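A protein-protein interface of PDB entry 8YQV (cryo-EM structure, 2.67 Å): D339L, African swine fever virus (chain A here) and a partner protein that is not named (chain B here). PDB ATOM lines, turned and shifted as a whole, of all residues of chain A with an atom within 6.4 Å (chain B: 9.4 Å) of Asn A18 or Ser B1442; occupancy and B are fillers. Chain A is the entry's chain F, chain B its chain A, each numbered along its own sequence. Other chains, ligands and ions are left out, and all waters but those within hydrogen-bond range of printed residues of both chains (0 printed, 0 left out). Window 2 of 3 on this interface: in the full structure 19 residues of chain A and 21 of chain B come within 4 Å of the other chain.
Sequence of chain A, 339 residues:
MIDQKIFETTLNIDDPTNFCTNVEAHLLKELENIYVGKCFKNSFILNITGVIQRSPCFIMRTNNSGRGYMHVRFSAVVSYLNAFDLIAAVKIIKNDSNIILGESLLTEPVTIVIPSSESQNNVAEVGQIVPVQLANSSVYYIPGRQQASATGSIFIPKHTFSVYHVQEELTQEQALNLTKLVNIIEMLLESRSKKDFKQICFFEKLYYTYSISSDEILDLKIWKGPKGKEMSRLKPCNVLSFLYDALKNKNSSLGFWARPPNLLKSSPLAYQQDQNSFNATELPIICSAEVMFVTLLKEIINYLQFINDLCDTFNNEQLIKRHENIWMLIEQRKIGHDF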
ATOM      1  N   ASP A  15     -17.294  -5.668  16.090  1.00  0.00           N
ATOM      2  CA  ASP A  15     -17.305  -6.921  15.337  1.00  0.00           C
ATOM      3  C   ASP A  15     -16.739  -6.644  13.960  1.00  0.00           C
ATOM      4  O   ASP A  15     -17.484  -6.471  12.989  1.00  0.00           O
ATOM      5  CB  ASP A  15     -18.713  -7.500  15.233  1.00  0.00           C
ATOM      6  CG  ASP A  15     -18.724  -8.911  14.696  1.00  0.00           C
ATOM      7  OD1 ASP A  15     -17.635  -9.491  14.516  1.00  0.00           O
ATOM      8  OD2 ASP A  15     -19.823  -9.441  14.445  1.00  0.00           O
ATOM      9  N   PRO A  16     -15.413  -6.585  13.834  1.00  0.00           N
ATOM     10  CA  PRO A  16     -14.824  -6.169  12.553  1.00  0.00           C
ATOM     11  C   PRO A  16     -15.189  -7.065  11.385  1.00  0.00           C
ATOM     12  O   PRO A  16     -15.375  -6.561  10.270  1.00  0.00           O
ATOM     13  CB  PRO A  16     -13.319  -6.203  12.840  1.00  0.00           C
ATOM     14  CG  PRO A  16     -13.210  -6.114  14.312  1.00  0.00           C
ATOM     15  CD  PRO A  16     -14.383  -6.848  14.848  1.00  0.00           C
ATOM     16  N   THR A  17     -15.306  -8.375  11.607  1.00  0.00           N
ATOM     17  CA  THR A  17     -15.594  -9.289  10.509  1.00  0.00           C
ATOM     18  C   THR A  17     -16.956  -9.011   9.893  1.00  0.00           C
ATOM     19  O   THR A  17     -17.105  -9.074   8.670  1.00  0.00           O
ATOM     20  CB  THR A  17     -15.518 -10.733  10.996  1.00  0.00           C
ATOM     21  OG1 THR A  17     -14.335 -10.910  11.779  1.00  0.00           O
ATOM     22  CG2 THR A  17     -15.467 -11.676   9.823  1.00  0.00           C
ATOM     23  N   ASN A  18     -17.957  -8.716  10.719  1.00  0.00           N
ATOM     24  CA  ASN A  18     -19.265  -8.339  10.202  1.00  0.00           C
ATOM     25  C   ASN A  18     -19.246  -6.944   9.597  1.00  0.00           C
ATOM     26  O   ASN A  18     -19.814  -6.725   8.524  1.00  0.00           O
ATOM     27  CB  ASN A  18     -20.309  -8.412  11.314  1.00  0.00           C
ATOM     28  CG  ASN A  18     -21.719  -8.267  10.795  1.00  0.00           C
ATOM     29  OD1 ASN A  18     -21.959  -8.307   9.591  1.00  0.00           O
ATOM     30  ND2 ASN A  18     -22.662  -8.077  11.704  1.00  0.00           N
ATOM     31  N   PHE A  19     -18.593  -5.996  10.269  1.00  0.00           N
ATOM     32  CA  PHE A  19     -18.577  -4.617   9.793  1.00  0.00           C
ATOM     33  C   PHE A  19     -17.978  -4.518   8.401  1.00  0.00           C
ATOM     34  O   PHE A  19     -18.440  -3.725   7.576  1.00  0.00           O
ATOM     35  CB  PHE A  19     -17.798  -3.741  10.771  1.00  0.00           C
ATOM     36  CG  PHE A  19     -17.843  -2.273  10.452  1.00  0.00           C
ATOM     37  CD1 PHE A  19     -18.794  -1.455  11.025  1.00  0.00           C
ATOM     38  CD2 PHE A  19     -16.923  -1.709   9.586  1.00  0.00           C
ATOM     39  CE1 PHE A  19     -18.828  -0.108  10.738  1.00  0.00           C
ATOM     40  CE2 PHE A  19     -16.959  -0.368   9.293  1.00  0.00           C
ATOM     41  CZ  PHE A  19     -17.911   0.432   9.869  1.00  0.00           C
ATOM     42  N   CYS A  20     -16.952  -5.312   8.117  1.00  0.00           N
ATOM     43  CA  CYS A  20     -16.258  -5.204   6.841  1.00  0.00           C
ATOM     44  C   CYS A  20     -16.989  -5.886   5.693  1.00  0.00           C
ATOM     45  O   CYS A  20     -16.532  -5.779   4.552  1.00  0.00           O
ATOM     46  CB  CYS A  20     -14.840  -5.766   6.968  1.00  0.00           C
ATOM     47  SG  CYS A  20     -13.718  -4.709   7.899  1.00  0.00           S
ATOM     48  N   THR A  21     -18.099  -6.580   5.951  1.00  0.00           N
ATOM     49  CA  THR A  21     -18.877  -7.144   4.853  1.00  0.00           C
ATOM     50  C   THR A  21     -19.525  -6.055   4.005  1.00  0.00           C
ATOM     51  O   THR A  21     -19.726  -6.248   2.803  1.00  0.00           O
ATOM     52  CB  THR A  21     -19.941  -8.101   5.387  1.00  0.00           C
ATOM     53  OG1 THR A  21     -20.810  -7.402   6.283  1.00  0.00           O
ATOM     54  CG2 THR A  21     -19.298  -9.255   6.120  1.00  0.00           C
ATOM     55  N   ASN A  22     -19.871  -4.920   4.613  1.00  0.00           N
ATOM     56  CA  ASN A  22     -20.332  -3.753   3.862  1.00  0.00           C
ATOM     57  C   ASN A  22     -19.904  -2.524   4.662  1.00  0.00           C
ATOM     58  O   ASN A  22     -20.624  -2.098   5.566  1.00  0.00           O
ATOM     59  CB  ASN A  22     -21.836  -3.789   3.652  1.00  0.00           C
ATOM     60  CG  ASN A  22     -22.318  -2.729   2.683  1.00  0.00           C
ATOM     61  OD1 ASN A  22     -21.541  -1.915   2.191  1.00  0.00           O
ATOM     62  ND2 ASN A  22     -23.612  -2.735   2.406  1.00  0.00           N
ATOM     63  N   HIS A  26     -22.559   0.156   6.844  1.00  0.00           N
ATOM     64  CA  HIS A  26     -22.344   0.111   8.284  1.00  0.00           C
ATOM     65  C   HIS A  26     -21.776   1.425   8.802  1.00  0.00           C
ATOM     66  O   HIS A  26     -22.144   1.876   9.893  1.00  0.00           O
ATOM     67  CB  HIS A  26     -21.413  -1.048   8.628  1.00  0.00           C
ATOM     68  CG  HIS A  26     -21.983  -2.398   8.326  1.00  0.00           C
ATOM     69  ND1 HIS A  26     -22.139  -2.870   7.041  1.00  0.00           N
ATOM     70  CD2 HIS A  26     -22.406  -3.390   9.142  1.00  0.00           C
ATOM     71  CE1 HIS A  26     -22.651  -4.085   7.078  1.00  0.00           C
ATOM     72  NE2 HIS A  26     -22.820  -4.426   8.341  1.00  0.00           N
ATOM     73  N   MET B1431      -8.096  -5.173   8.535  1.00  0.00           N
ATOM     74  CA  MET B1431      -9.046  -6.181   8.093  1.00  0.00           C
ATOM     75  C   MET B1431      -9.116  -6.177   6.573  1.00  0.00           C
ATOM     76  O   MET B1431      -9.228  -5.114   5.954  1.00  0.00           O
ATOM     77  CB  MET B1431     -10.426  -5.915   8.692  1.00  0.00           C
ATOM     78  CG  MET B1431     -10.464  -6.008  10.205  1.00  0.00           C
ATOM     79  SD  MET B1431     -10.737  -7.636  10.906  1.00  0.00           S
ATOM     80  CE  MET B1431     -11.496  -8.475   9.539  1.00  0.00           C
ATOM     81  N   GLU B1433     -10.874  -6.107   3.650  1.00  0.00           N
ATOM     82  CA  GLU B1433     -12.236  -5.846   3.200  1.00  0.00           C
ATOM     83  C   GLU B1433     -12.534  -6.555   1.888  1.00  0.00           C
ATOM     84  O   GLU B1433     -13.596  -7.164   1.734  1.00  0.00           O
ATOM     85  CB  GLU B1433     -12.451  -4.344   3.046  1.00  0.00           C
ATOM     86  CG  GLU B1433     -12.083  -3.529   4.265  1.00  0.00           C
ATOM     87  CD  GLU B1433     -12.089  -2.043   3.983  1.00  0.00           C
ATOM     88  OE1 GLU B1433     -12.367  -1.658   2.829  1.00  0.00           O
ATOM     89  OE2 GLU B1433     -11.811  -1.256   4.912  1.00  0.00           O
ATOM     90  N   ILE B1436     -13.405 -10.150   2.444  1.00  0.00           N
ATOM     91  CA  ILE B1436     -14.568 -10.460   3.264  1.00  0.00           C
ATOM     92  C   ILE B1436     -15.863 -10.147   2.529  1.00  0.00           C
ATOM     93  O   ILE B1436     -16.844 -10.885   2.659  1.00  0.00           O
ATOM     94  CB  ILE B1436     -14.473  -9.709   4.599  1.00  0.00           C
ATOM     95  CG1 ILE B1436     -13.337 -10.282   5.430  1.00  0.00           C
ATOM     96  CG2 ILE B1436     -15.756  -9.815   5.372  1.00  0.00           C
ATOM     97  CD1 ILE B1436     -13.014  -9.461   6.612  1.00  0.00           C
ATOM     98  N   THR B1437     -15.901  -9.071   1.744  1.00  0.00           N
ATOM     99  CA  THR B1437     -17.105  -8.768   0.984  1.00  0.00           C
ATOM    100  C   THR B1437     -17.388  -9.811  -0.087  1.00  0.00           C
ATOM    101  O   THR B1437     -18.539  -9.936  -0.521  1.00  0.00           O
ATOM    102  CB  THR B1437     -17.002  -7.392   0.330  1.00  0.00           C
ATOM    103  OG1 THR B1437     -15.930  -7.391  -0.619  1.00  0.00           O
ATOM    104  CG2 THR B1437     -16.738  -6.328   1.371  1.00  0.00           C
ATOM    105  N   ASN B1439     -16.473 -13.176   0.294  1.00  0.00           N
ATOM    106  CA  ASN B1439     -16.496 -14.510   0.878  1.00  0.00           C
ATOM    107  C   ASN B1439     -17.426 -14.655   2.069  1.00  0.00           C
ATOM    108  O   ASN B1439     -17.826 -15.784   2.372  1.00  0.00           O
ATOM    109  CB  ASN B1439     -15.082 -14.937   1.304  1.00  0.00           C
ATOM    110  CG  ASN B1439     -14.171 -15.203   0.120  1.00  0.00           C
ATOM    111  OD1 ASN B1439     -13.302 -14.398  -0.202  1.00  0.00           O
ATOM    112  ND2 ASN B1439     -14.366 -16.339  -0.534  1.00  0.00           N
ATOM    113  N   TYR B1440     -17.778 -13.574   2.756  1.00  0.00           N
ATOM    114  CA  TYR B1440     -18.642 -13.635   3.924  1.00  0.00           C
ATOM    115  C   TYR B1440     -19.943 -12.897   3.632  1.00  0.00           C
ATOM    116  O   TYR B1440     -20.069 -12.168   2.646  1.00  0.00           O
ATOM    117  CB  TYR B1440     -17.965 -13.035   5.169  1.00  0.00           C
ATOM    118  CG  TYR B1440     -16.726 -13.755   5.684  1.00  0.00           C
ATOM    119  CD1 TYR B1440     -16.357 -13.661   7.015  1.00  0.00           C
ATOM    120  CD2 TYR B1440     -15.917 -14.498   4.847  1.00  0.00           C
ATOM    121  CE1 TYR B1440     -15.233 -14.302   7.490  1.00  0.00           C
ATOM    122  CE2 TYR B1440     -14.796 -15.135   5.312  1.00  0.00           C
ATOM    123  CZ  TYR B1440     -14.459 -15.038   6.631  1.00  0.00           C
ATOM    124  OH  TYR B1440     -13.334 -15.680   7.086  1.00  0.00           O
ATOM    125  N   LYS B1441     -20.922 -13.098   4.510  1.00  0.00           N
ATOM    126  CA  LYS B1441     -22.209 -12.429   4.404  1.00  0.00           C
ATOM    127  C   LYS B1441     -22.604 -11.899   5.775  1.00  0.00           C
ATOM    128  O   LYS B1441     -22.185 -12.423   6.810  1.00  0.00           O
ATOM    129  CB  LYS B1441     -23.292 -13.369   3.856  1.00  0.00           C
ATOM    130  CG  LYS B1441     -23.634 -14.527   4.777  1.00  0.00           C
ATOM    131  CD  LYS B1441     -24.524 -15.542   4.083  1.00  0.00           C
ATOM    132  CE  LYS B1441     -25.927 -15.004   3.871  1.00  0.00           C
ATOM    133  NZ  LYS B1441     -26.824 -16.030   3.268  1.00  0.00           N
ATOM    134  N   SER B1442     -23.410 -10.843   5.771  1.00  0.00           N
ATOM    135  CA  SER B1442     -23.848 -10.221   7.014  1.00  0.00           C
ATOM    136  C   SER B1442     -24.835 -11.115   7.758  1.00  0.00           C
ATOM    137  O   SER B1442     -24.501 -11.708   8.783  1.00  0.00           O
ATOM    138  CB  SER B1442     -24.479  -8.854   6.740  1.00  0.00           C
ATOM    139  OG  SER B1442     -23.519  -7.935   6.250  1.00  0.00           O
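O of Glu B1433 sits close to OG1 of Thr B1437.
The side-chain sulfur (SG) of Cys A20 lies within hydrogen-bond range of the backbone carbonyl oxygen (O) of Pro A16 (3.4 Å).
The backbone carbonyl oxygen (O) of Asn A18 sits at hydrogen-bond distance from the side-chain hydroxyl (OG1) of Thr A21 (2.5 Å).
Printed residues of chain A that touch a printed residue of chain B: Pro A16, Thr A17, Asn A18, Cys A20 and Thr A21.
Printed residues of chain B that touch a printed residue of chain A: Met B1431, Ile B1436, Thr B1437, Tyr B1440 and Ser B1442.
Among the printed residues, 9 pairs touch across the chains.
Among the printed residues, no Asp or Glu carboxylate lies within 4 Å of a Lys or Arg side-chain nitrogen of the other chain.
Among the printed residues, pairs that only touch across the chains: Pro A16 with Met B1431, Thr A17 with Ile B1436, Thr A17 with Tyr B1440, Asn A18 with Ser B1442, Cys A20 with Met B1431, Cys A20 with Thr B1437, Thr A21 with Ile B1436 and Thr A21 with Thr B1437.
Of chain B, only Ser B1442 (3.7 Å) comes within 4 Å of Asn A18.
Printed residues of chain A within 4 Å of Ser B1442: Asn A18 (3.7 Å) and Thr A21 (2.8 Å).
Thr A17 touches just these residues of chain B: Ile B1436 (3.6 Å) and Tyr B1440 (3.5 Å).
Of the printed residues of chain A, Ile B1436 touches Thr A17 (3.6 Å) and Thr A21 (3.7 Å).
Of the printed residues of chain A, Met B1431 touches Pro A16 (3.5 Å) and Cys A20 (3.6 Å).
Of the printed residues of chain A, Tyr B1440 touches Thr A17 (3.5 Å).
The nearest residue of chain B that does not touch Asn A18 is Lys B1441 (5.0 Å).
The nearest printed residue of chain B that does not touch Cys A20 is Ile B1436 (4.1 Å).
The side-chain hydroxyl (OG1) of Thr A21 sits at hydrogen-bond distance from the side-chain hydroxyl (OG) of Ser B1442 (2.8 Å).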
